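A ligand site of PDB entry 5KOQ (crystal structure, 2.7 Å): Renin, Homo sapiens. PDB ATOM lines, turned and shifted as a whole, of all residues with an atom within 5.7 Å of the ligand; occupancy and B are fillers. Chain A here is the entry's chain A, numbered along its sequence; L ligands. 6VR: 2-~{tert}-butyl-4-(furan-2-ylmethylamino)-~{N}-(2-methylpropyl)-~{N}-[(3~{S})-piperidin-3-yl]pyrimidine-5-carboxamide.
N20 of the ligand sits at hydrogen-bond distance from O of Gly 225, 2.7 Å away. A nitrogen (N10) of the ligand is in salt-bridge range of the side-chain carboxylate of Asp 223 (2.8 Å). N10 of the ligand lies within salt-bridge range of OD1 of Asp 35 (2.9 Å). A nitrogen (N16) of the ligand lies close to the side-chain hydroxyl of Thr 82 (3.4 Å). An oxygen (O26) of the ligand lies within hydrogen-bond range of the backbone NH (N) of Ser 227 (3.3 Å).
N of Gly 225 is in hydrogen-bond range of OD1 of Asp 223 (3.0 Å). The side-chain carboxylate (OD1) of Asp 223 lies close to the side-chain carboxylate (OD1) of Asp 35 (2.6 Å). The backbone NH (N) of Gly 37 lies within hydrogen-bond range of the side-chain carboxylate (OD1) of Asp 35 (2.8 Å). OD2 of Asp 35 sits at hydrogen-bond distance from OG of Ser 38 (2.8 Å). The backbone NH (N) of Ala 314 sits at hydrogen-bond distance from the backbone carbonyl oxygen (O) of Ala 226 (2.8 Å). The side-chain hydroxyl (OH) of Tyr 159 lies within hydrogen-bond range of the backbone carbonyl oxygen (O) of Thr 224. NE2 of Gln 16 lies within hydrogen-bond range of O of Leu 118, 2.8 Å away. The side-chain hydroxyl (OH) of Tyr 80 sits at hydrogen-bond distance from the indole nitrogen (NE1) of Trp 42, 2.8 Å away.
The backbone carbonyl oxygen (O) of Thr 15 lies close to an oxygen (O26) of the ligand, at 3.1 Å. O26 of the ligand lies close to O of Ala 226, at 3.3 Å. Residues that only touch the ligand: Gln 16, Tyr 17, Val 33, Gly 37, Tyr 80, Ser 81, Pro 115, Phe 116, Leu 118, Ala 119, Phe 121, Val 124, Tyr 159 and Thr 224. Hydrophobic or aromatic side chains that line the ligand: Tyr 17, Val 33, Tyr 80, Pro 115, Phe 116, Ala 119, Phe 121, Val 124 and Ala 226. The nearest printed residue that does not touch the ligand is Ala 314 (4.3 Å).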
ATOM      1  N   THR A  15     -31.530 -10.573   2.846  1.00  0.00           N
ATOM      2  CA  THR A  15     -30.631  -9.478   3.240  1.00  0.00           C
ATOM      3  C   THR A  15     -29.410  -9.968   4.016  1.00  0.00           C
ATOM      4  O   THR A  15     -28.385  -9.303   4.033  1.00  0.00           O
ATOM      5  CB  THR A  15     -31.357  -8.396   4.056  1.00  0.00           C
ATOM      6  OG1 THR A  15     -32.048  -9.000   5.153  1.00  0.00           O
ATOM      7  CG2 THR A  15     -32.357  -7.620   3.190  1.00  0.00           C
ATOM      8  N   GLN A  16     -29.537 -11.125   4.654  1.00  0.00           N
ATOM      9  CA  GLN A  16     -28.458 -11.668   5.445  1.00  0.00           C
ATOM     10  C   GLN A  16     -28.194 -13.120   5.077  1.00  0.00           C
ATOM     11  O   GLN A  16     -29.066 -13.989   5.228  1.00  0.00           O
ATOM     12  CB  GLN A  16     -28.777 -11.538   6.922  1.00  0.00           C
ATOM     13  CG  GLN A  16     -28.803 -10.115   7.441  1.00  0.00           C
ATOM     14  CD  GLN A  16     -29.005 -10.061   8.931  1.00  0.00           C
ATOM     15  OE1 GLN A  16     -28.269 -10.676   9.691  1.00  0.00           O
ATOM     16  NE2 GLN A  16     -30.017  -9.321   9.363  1.00  0.00           N
ATOM     17  N   TYR A  17     -26.993 -13.369   4.572  1.00  0.00           N
ATOM     18  CA  TYR A  17     -26.539 -14.704   4.177  1.00  0.00           C
ATOM     19  C   TYR A  17     -25.325 -15.054   4.997  1.00  0.00           C
ATOM     20  O   TYR A  17     -24.331 -14.313   5.016  1.00  0.00           O
ATOM     21  CB  TYR A  17     -26.183 -14.736   2.696  1.00  0.00           C
ATOM     22  CG  TYR A  17     -27.345 -14.589   1.748  1.00  0.00           C
ATOM     23  CD1 TYR A  17     -27.852 -13.324   1.417  1.00  0.00           C
ATOM     24  CD2 TYR A  17     -27.939 -15.720   1.178  1.00  0.00           C
ATOM     25  CE1 TYR A  17     -28.922 -13.184   0.545  1.00  0.00           C
ATOM     26  CE2 TYR A  17     -29.001 -15.587   0.296  1.00  0.00           C
ATOM     27  CZ  TYR A  17     -29.499 -14.326  -0.014  1.00  0.00           C
ATOM     28  OH  TYR A  17     -30.553 -14.198  -0.886  1.00  0.00           O
ATOM     29  N   TYR A  18     -25.409 -16.183   5.689  1.00  0.00           N
ATOM     30  CA  TYR A  18     -24.345 -16.593   6.596  1.00  0.00           C
ATOM     31  C   TYR A  18     -24.251 -18.113   6.700  1.00  0.00           C
ATOM     32  O   TYR A  18     -25.235 -18.815   6.504  1.00  0.00           O
ATOM     33  CB  TYR A  18     -24.547 -15.969   7.983  1.00  0.00           C
ATOM     34  CG  TYR A  18     -25.900 -16.259   8.605  1.00  0.00           C
ATOM     35  CD1 TYR A  18     -26.104 -17.429   9.340  1.00  0.00           C
ATOM     36  CD2 TYR A  18     -26.974 -15.383   8.438  1.00  0.00           C
ATOM     37  CE1 TYR A  18     -27.334 -17.709   9.903  1.00  0.00           C
ATOM     38  CE2 TYR A  18     -28.212 -15.657   9.001  1.00  0.00           C
ATOM     39  CZ  TYR A  18     -28.389 -16.824   9.724  1.00  0.00           C
ATOM     40  OH  TYR A  18     -29.600 -17.129  10.299  1.00  0.00           O
ATOM     41  N   VAL A  33     -20.827 -14.109   8.214  1.00  0.00           N
ATOM     42  CA  VAL A  33     -20.956 -13.618   6.857  1.00  0.00           C
ATOM     43  C   VAL A  33     -19.619 -13.814   6.156  1.00  0.00           C
ATOM     44  O   VAL A  33     -18.580 -13.370   6.654  1.00  0.00           O
ATOM     45  CB  VAL A  33     -21.349 -12.126   6.804  1.00  0.00           C
ATOM     46  CG1 VAL A  33     -21.351 -11.619   5.368  1.00  0.00           C
ATOM     47  CG2 VAL A  33     -22.715 -11.923   7.416  1.00  0.00           C
ATOM     48  N   ASP A  35     -17.581 -12.477   3.504  1.00  0.00           N
ATOM     49  CA  ASP A  35     -17.628 -11.133   2.954  1.00  0.00           C
ATOM     50  C   ASP A  35     -16.410 -10.834   2.076  1.00  0.00           C
ATOM     51  O   ASP A  35     -15.291 -10.682   2.566  1.00  0.00           O
ATOM     52  CB  ASP A  35     -17.774 -10.132   4.119  1.00  0.00           C
ATOM     53  CG  ASP A  35     -17.721  -8.668   3.679  1.00  0.00           C
ATOM     54  OD1 ASP A  35     -18.048  -8.361   2.509  1.00  0.00           O
ATOM     55  OD2 ASP A  35     -17.351  -7.815   4.519  1.00  0.00           O
ATOM     56  N   GLY A  37     -15.962  -8.110   0.657  1.00  0.00           N
ATOM     57  CA  GLY A  37     -15.747  -6.669   0.806  1.00  0.00           C
ATOM     58  C   GLY A  37     -14.891  -6.285   1.989  1.00  0.00           C
ATOM     59  O   GLY A  37     -14.605  -5.095   2.186  1.00  0.00           O
ATOM     60  N   SER A  38     -14.505  -7.273   2.797  1.00  0.00           N
ATOM     61  CA  SER A  38     -13.540  -7.080   3.876  1.00  0.00           C
ATOM     62  C   SER A  38     -12.617  -8.290   3.943  1.00  0.00           C
ATOM     63  O   SER A  38     -12.833  -9.265   3.230  1.00  0.00           O
ATOM     64  CB  SER A  38     -14.227  -6.827   5.228  1.00  0.00           C
ATOM     65  OG  SER A  38     -14.872  -7.993   5.706  1.00  0.00           O
ATOM     66  N   TRP A  42     -13.737 -11.873  12.335  1.00  0.00           N
ATOM     67  CA  TRP A  42     -14.091 -11.530  13.706  1.00  0.00           C
ATOM     68  C   TRP A  42     -15.355 -12.222  14.162  1.00  0.00           C
ATOM     69  O   TRP A  42     -16.276 -12.475  13.380  1.00  0.00           O
ATOM     70  CB  TRP A  42     -14.195 -10.008  13.935  1.00  0.00           C
ATOM     71  CG  TRP A  42     -15.363  -9.330  13.233  1.00  0.00           C
ATOM     72  CD1 TRP A  42     -15.332  -8.722  12.014  1.00  0.00           C
ATOM     73  CD2 TRP A  42     -16.704  -9.166  13.727  1.00  0.00           C
ATOM     74  NE1 TRP A  42     -16.565  -8.191  11.718  1.00  0.00           N
ATOM     75  CE2 TRP A  42     -17.426  -8.460  12.743  1.00  0.00           C
ATOM     76  CE3 TRP A  42     -17.358  -9.570  14.897  1.00  0.00           C
ATOM     77  CZ2 TRP A  42     -18.793  -8.132  12.894  1.00  0.00           C
ATOM     78  CZ3 TRP A  42     -18.724  -9.240  15.059  1.00  0.00           C
ATOM     79  CH2 TRP A  42     -19.413  -8.525  14.051  1.00  0.00           C
ATOM     80  N   TYR A  80     -16.526  -0.543   9.079  1.00  0.00           N
ATOM     81  CA  TYR A  80     -17.326  -0.790   7.906  1.00  0.00           C
ATOM     82  C   TYR A  80     -18.144   0.465   7.605  1.00  0.00           C
ATOM     83  O   TYR A  80     -18.264   1.353   8.450  1.00  0.00           O
ATOM     84  CB  TYR A  80     -18.230  -1.995   8.111  1.00  0.00           C
ATOM     85  CG  TYR A  80     -17.497  -3.273   8.490  1.00  0.00           C
ATOM     86  CD1 TYR A  80     -16.763  -3.988   7.547  1.00  0.00           C
ATOM     87  CD2 TYR A  80     -17.563  -3.775   9.799  1.00  0.00           C
ATOM     88  CE1 TYR A  80     -16.096  -5.158   7.886  1.00  0.00           C
ATOM     89  CE2 TYR A  80     -16.909  -4.945  10.150  1.00  0.00           C
ATOM     90  CZ  TYR A  80     -16.174  -5.626   9.192  1.00  0.00           C
ATOM     91  OH  TYR A  80     -15.522  -6.784   9.531  1.00  0.00           O
ATOM     92  N   SER A  81     -18.700   0.521   6.399  1.00  0.00           N
ATOM     93  CA  SER A  81     -19.553   1.624   5.948  1.00  0.00           C
ATOM     94  C   SER A  81     -20.828   1.807   6.779  1.00  0.00           C
ATOM     95  O   SER A  81     -21.371   2.911   6.834  1.00  0.00           O
ATOM     96  CB  SER A  81     -19.894   1.453   4.465  1.00  0.00           C
ATOM     97  OG  SER A  81     -20.468   0.179   4.185  1.00  0.00           O
ATOM     98  N   THR A  82     -21.309   0.731   7.407  1.00  0.00           N
ATOM     99  CA  THR A  82     -22.606   0.716   8.102  1.00  0.00           C
ATOM    100  C   THR A  82     -22.450   0.745   9.634  1.00  0.00           C
ATOM    101  O   THR A  82     -23.447   0.810  10.362  1.00  0.00           O
ATOM    102  CB  THR A  82     -23.458  -0.514   7.722  1.00  0.00           C
ATOM    103  OG1 THR A  82     -22.993  -1.667   8.445  1.00  0.00           O
ATOM    104  CG2 THR A  82     -23.407  -0.800   6.211  1.00  0.00           C
ATOM    105  N   PRO A 115     -25.535  -1.170  14.320  1.00  0.00           N
ATOM    106  CA  PRO A 115     -26.590  -1.970  13.676  1.00  0.00           C
ATOM    107  C   PRO A 115     -26.656  -3.435  14.126  1.00  0.00           C
ATOM    108  O   PRO A 115     -27.485  -4.196  13.615  1.00  0.00           O
ATOM    109  CB  PRO A 115     -26.161  -1.940  12.213  1.00  0.00           C
ATOM    110  CG  PRO A 115     -24.667  -1.960  12.277  1.00  0.00           C
ATOM    111  CD  PRO A 115     -24.299  -1.141  13.505  1.00  0.00           C
ATOM    112  N   PHE A 116     -25.791  -3.839  15.064  1.00  0.00           N
ATOM    113  CA  PHE A 116     -25.525  -5.262  15.248  1.00  0.00           C
ATOM    114  C   PHE A 116     -26.596  -6.120  15.904  1.00  0.00           C
ATOM    115  O   PHE A 116     -26.622  -7.332  15.705  1.00  0.00           O
ATOM    116  CB  PHE A 116     -24.103  -5.501  15.788  1.00  0.00           C
ATOM    117  CG  PHE A 116     -23.035  -5.157  14.793  1.00  0.00           C
ATOM    118  CD1 PHE A 116     -22.758  -6.014  13.723  1.00  0.00           C
ATOM    119  CD2 PHE A 116     -22.347  -3.941  14.872  1.00  0.00           C
ATOM    120  CE1 PHE A 116     -21.800  -5.680  12.776  1.00  0.00           C
ATOM    121  CE2 PHE A 116     -21.391  -3.593  13.922  1.00  0.00           C
ATOM    122  CZ  PHE A 116     -21.116  -4.469  12.875  1.00  0.00           C
ATOM    123  N   LEU A 118     -29.447  -6.032  14.741  1.00  0.00           N
ATOM    124  CA  LEU A 118     -30.193  -6.438  13.554  1.00  0.00           C
ATOM    125  C   LEU A 118     -29.562  -7.624  12.827  1.00  0.00           C
ATOM    126  O   LEU A 118     -30.192  -8.210  11.929  1.00  0.00           O
ATOM    127  CB  LEU A 118     -30.401  -5.257  12.600  1.00  0.00           C
ATOM    128  CG  LEU A 118     -31.115  -3.992  13.120  1.00  0.00           C
ATOM    129  CD1 LEU A 118     -30.970  -2.846  12.129  1.00  0.00           C
ATOM    130  CD2 LEU A 118     -32.590  -4.244  13.411  1.00  0.00           C
ATOM    131  N   ALA A 119     -28.329  -7.986  13.213  1.00  0.00           N
ATOM    132  CA  ALA A 119     -27.592  -9.093  12.602  1.00  0.00           C
ATOM    133  C   ALA A 119     -28.060 -10.438  13.132  1.00  0.00           C
ATOM    134  O   ALA A 119     -28.082 -10.672  14.344  1.00  0.00           O
ATOM    135  CB  ALA A 119     -26.093  -8.934  12.835  1.00  0.00           C
ATOM    136  N   GLU A 120     -28.441 -11.308  12.214  1.00  0.00           N
ATOM    137  CA  GLU A 120     -28.699 -12.700  12.525  1.00  0.00           C
ATOM    138  C   GLU A 120     -27.387 -13.444  12.753  1.00  0.00           C
ATOM    139  O   GLU A 120     -27.295 -14.338  13.597  1.00  0.00           O
ATOM    140  CB  GLU A 120     -29.512 -13.371  11.427  1.00  0.00           C
ATOM    141  CG  GLU A 120     -31.017 -13.318  11.651  1.00  0.00           C
ATOM    142  CD  GLU A 120     -31.450 -14.055  12.911  1.00  0.00           C
ATOM    143  OE1 GLU A 120     -30.918 -15.158  13.179  1.00  0.00           O
ATOM    144  OE2 GLU A 120     -32.299 -13.517  13.641  1.00  0.00           O
ATOM    145  N   PHE A 121     -26.374 -13.046  11.976  1.00  0.00           N
ATOM    146  CA  PHE A 121     -25.031 -13.591  12.085  1.00  0.00           C
ATOM    147  C   PHE A 121     -24.336 -13.035  13.327  1.00  0.00           C
ATOM    148  O   PHE A 121     -24.686 -11.955  13.807  1.00  0.00           O
ATOM    149  CB  PHE A 121     -24.226 -13.257  10.824  1.00  0.00           C
ATOM    150  CG  PHE A 121     -24.173 -11.789  10.475  1.00  0.00           C
ATOM    151  CD1 PHE A 121     -25.166 -11.199   9.672  1.00  0.00           C
ATOM    152  CD2 PHE A 121     -23.098 -10.990  10.906  1.00  0.00           C
ATOM    153  CE1 PHE A 121     -25.119  -9.853   9.339  1.00  0.00           C
ATOM    154  CE2 PHE A 121     -23.045  -9.635  10.571  1.00  0.00           C
ATOM    155  CZ  PHE A 121     -24.048  -9.074   9.782  1.00  0.00           C
ATOM    156  N   VAL A 124     -17.989 -12.057  11.088  1.00  0.00           N
ATOM    157  CA  VAL A 124     -17.646 -11.941   9.670  1.00  0.00           C
ATOM    158  C   VAL A 124     -16.394 -12.755   9.364  1.00  0.00           C
ATOM    159  O   VAL A 124     -15.407 -12.713  10.107  1.00  0.00           O
ATOM    160  CB  VAL A 124     -17.452 -10.456   9.239  1.00  0.00           C
ATOM    161  CG1 VAL A 124     -17.014 -10.331   7.784  1.00  0.00           C
ATOM    162  CG2 VAL A 124     -18.725  -9.640   9.465  1.00  0.00           C
ATOM    163  N   TYR A 159     -26.220 -17.439  -3.928  1.00  0.00           N
ATOM    164  CA  TYR A 159     -27.226 -16.898  -2.997  1.00  0.00           C
ATOM    165  C   TYR A 159     -28.606 -17.164  -3.548  1.00  0.00           C
ATOM    166  O   TYR A 159     -28.957 -16.686  -4.637  1.00  0.00           O
ATOM    167  CB  TYR A 159     -27.050 -15.389  -2.773  1.00  0.00           C
ATOM    168  CG  TYR A 159     -25.933 -14.955  -1.835  1.00  0.00           C
ATOM    169  CD1 TYR A 159     -25.169 -15.881  -1.118  1.00  0.00           C
ATOM    170  CD2 TYR A 159     -25.655 -13.594  -1.639  1.00  0.00           C
ATOM    171  CE1 TYR A 159     -24.161 -15.478  -0.259  1.00  0.00           C
ATOM    172  CE2 TYR A 159     -24.649 -13.178  -0.782  1.00  0.00           C
ATOM    173  CZ  TYR A 159     -23.904 -14.130  -0.091  1.00  0.00           C
ATOM    174  OH  TYR A 159     -22.904 -13.737   0.759  1.00  0.00           O
ATOM    175  N   LEU A 221     -17.435  -2.645  -6.646  1.00  0.00           N
ATOM    176  CA  LEU A 221     -17.006  -3.651  -5.677  1.00  0.00           C
ATOM    177  C   LEU A 221     -18.016  -4.789  -5.635  1.00  0.00           C
ATOM    178  O   LEU A 221     -19.213  -4.568  -5.490  1.00  0.00           O
ATOM    179  CB  LEU A 221     -16.887  -3.018  -4.279  1.00  0.00           C
ATOM    180  CG  LEU A 221     -16.403  -3.895  -3.128  1.00  0.00           C
ATOM    181  CD1 LEU A 221     -14.882  -3.913  -3.085  1.00  0.00           C
ATOM    182  CD2 LEU A 221     -16.978  -3.414  -1.801  1.00  0.00           C
ATOM    183  N   ASP A 223     -19.406  -7.477  -3.558  1.00  0.00           N
ATOM    184  CA  ASP A 223     -19.446  -7.526  -2.096  1.00  0.00           C
ATOM    185  C   ASP A 223     -20.511  -8.516  -1.585  1.00  0.00           C
ATOM    186  O   ASP A 223     -21.663  -8.132  -1.332  1.00  0.00           O
ATOM    187  CB  ASP A 223     -19.668  -6.111  -1.534  1.00  0.00           C
ATOM    188  CG  ASP A 223     -19.568  -6.038   0.006  1.00  0.00           C
ATOM    189  OD1 ASP A 223     -19.450  -7.069   0.694  1.00  0.00           O
ATOM    190  OD2 ASP A 223     -19.614  -4.904   0.543  1.00  0.00           O
ATOM    191  N   THR A 224     -20.082  -9.757  -1.394  1.00  0.00           N
ATOM    192  CA  THR A 224     -20.954 -10.841  -0.933  1.00  0.00           C
ATOM    193  C   THR A 224     -21.500 -10.599   0.473  1.00  0.00           C
ATOM    194  O   THR A 224     -22.475 -11.228   0.893  1.00  0.00           O
ATOM    195  CB  THR A 224     -20.226 -12.195  -0.947  1.00  0.00           C
ATOM    196  OG1 THR A 224     -19.112 -12.161  -0.049  1.00  0.00           O
ATOM    197  CG2 THR A 224     -19.752 -12.548  -2.355  1.00  0.00           C
ATOM    198  N   GLY A 225     -20.864  -9.667   1.186  1.00  0.00           N
ATOM    199  CA  GLY A 225     -21.238  -9.334   2.560  1.00  0.00           C
ATOM    200  C   GLY A 225     -22.270  -8.241   2.656  1.00  0.00           C
ATOM    201  O   GLY A 225     -22.726  -7.929   3.754  1.00  0.00           O
ATOM    202  N   ALA A 226     -22.643  -7.664   1.515  1.00  0.00           N
ATOM    203  CA  ALA A 226     -23.655  -6.603   1.442  1.00  0.00           C
ATOM    204  C   ALA A 226     -24.997  -7.159   1.007  1.00  0.00           C
ATOM    205  O   ALA A 226     -25.060  -8.103   0.200  1.00  0.00           O
ATOM    206  CB  ALA A 226     -23.203  -5.497   0.489  1.00  0.00           C
ATOM    207  N   SER A 227     -26.071  -6.594   1.555  1.00  0.00           N
ATOM    208  CA  SER A 227     -27.434  -6.976   1.220  1.00  0.00           C
ATOM    209  C   SER A 227     -27.833  -6.526  -0.176  1.00  0.00           C
ATOM    210  O   SER A 227     -28.520  -7.245  -0.913  1.00  0.00           O
ATOM    211  CB  SER A 227     -28.409  -6.358   2.220  1.00  0.00           C
ATOM    212  OG  SER A 227     -28.127  -6.784   3.529  1.00  0.00           O
ATOM    213  N   MET A 300     -24.724   4.156  -0.159  1.00  0.00           N
ATOM    214  CA  MET A 300     -23.618   3.733   0.716  1.00  0.00           C
ATOM    215  C   MET A 300     -22.339   4.394   0.213  1.00  0.00           C
ATOM    216  O   MET A 300     -21.805   4.021  -0.822  1.00  0.00           O
ATOM    217  CB  MET A 300     -23.491   2.190   0.761  1.00  0.00           C
ATOM    218  CG  MET A 300     -22.535   1.646   1.812  1.00  0.00           C
ATOM    219  SD  MET A 300     -22.728  -0.123   2.147  1.00  0.00           S
ATOM    220  CE  MET A 300     -21.711  -0.894   0.891  1.00  0.00           C
ATOM    221  N   ALA A 314     -25.949  -8.809  -2.334  1.00  0.00           N
ATOM    222  CA  ALA A 314     -26.820  -9.972  -2.479  1.00  0.00           C
ATOM    223  C   ALA A 314     -27.925  -9.835  -3.530  1.00  0.00           C
ATOM    224  O   ALA A 314     -28.289 -10.835  -4.160  1.00  0.00           O
ATOM    225  CB  ALA A 314     -27.396 -10.380  -1.131  1.00  0.00           C
HETATM  226  C4  6VR L   1     -21.052  -5.136   7.130  1.00  0.00           C
HETATM  227  C6  6VR L   1     -20.624  -4.714   4.608  1.00  0.00           C
HETATM  228  C7  6VR L   1     -19.610  -3.602   4.953  1.00  0.00           C
HETATM  229  C8  6VR L   1     -18.644  -3.350   3.783  1.00  0.00           C
HETATM  230  C15 6VR L   1     -24.117  -4.287   7.438  1.00  0.00           C
HETATM  231  C17 6VR L   1     -25.861  -5.469   8.378  1.00  0.00           C
HETATM  232  C21 6VR L   1     -25.522  -8.644   5.667  1.00  0.00           C
HETATM  233  C22 6VR L   1     -25.237  -9.594   4.528  1.00  0.00           C
HETATM  234  C24 6VR L   1     -24.694 -11.378   3.336  1.00  0.00           C
HETATM  235  C28 6VR L   1     -26.184  -5.691  10.828  1.00  0.00           C
HETATM  236  C1  6VR L   1     -21.343  -7.726   7.069  1.00  0.00           C
HETATM  237  C2  6VR L   1     -20.615  -6.516   7.661  1.00  0.00           C
HETATM  238  C3  6VR L   1     -20.822  -6.515   9.187  1.00  0.00           C
HETATM  239  N5  6VR L   1     -21.555  -4.987   5.738  1.00  0.00           N
HETATM  240  C9  6VR L   1     -17.903  -4.652   3.458  1.00  0.00           C
HETATM  241  N10 6VR L   1     -18.894  -5.686   3.082  1.00  0.00           N
HETATM  242  C11 6VR L   1     -19.915  -5.984   4.109  1.00  0.00           C
HETATM  243  C12 6VR L   1     -22.886  -5.046   5.431  1.00  0.00           C
HETATM  244  O13 6VR L   1     -23.270  -4.895   4.284  1.00  0.00           O
HETATM  245  C14 6VR L   1     -23.946  -5.263   6.450  1.00  0.00           C
HETATM  246  N16 6VR L   1     -25.051  -4.426   8.370  1.00  0.00           N
HETATM  247  N18 6VR L   1     -25.755  -6.411   7.450  1.00  0.00           N
HETATM  248  C19 6VR L   1     -24.833  -6.373   6.471  1.00  0.00           C
HETATM  249  N20 6VR L   1     -24.755  -7.386   5.524  1.00  0.00           N
HETATM  250  C23 6VR L   1     -24.831 -10.868   4.653  1.00  0.00           C
HETATM  251  C25 6VR L   1     -25.026 -10.386   2.494  1.00  0.00           C
HETATM  252  O26 6VR L   1     -25.359  -9.305   3.216  1.00  0.00           O
HETATM  253  C27 6VR L   1     -26.897  -5.551   9.480  1.00  0.00           C
HETATM  254  C29 6VR L   1     -27.785  -4.292   9.486  1.00  0.00           C
HETATM  255  C30 6VR L   1     -27.811  -6.770   9.334  1.00  0.00           C
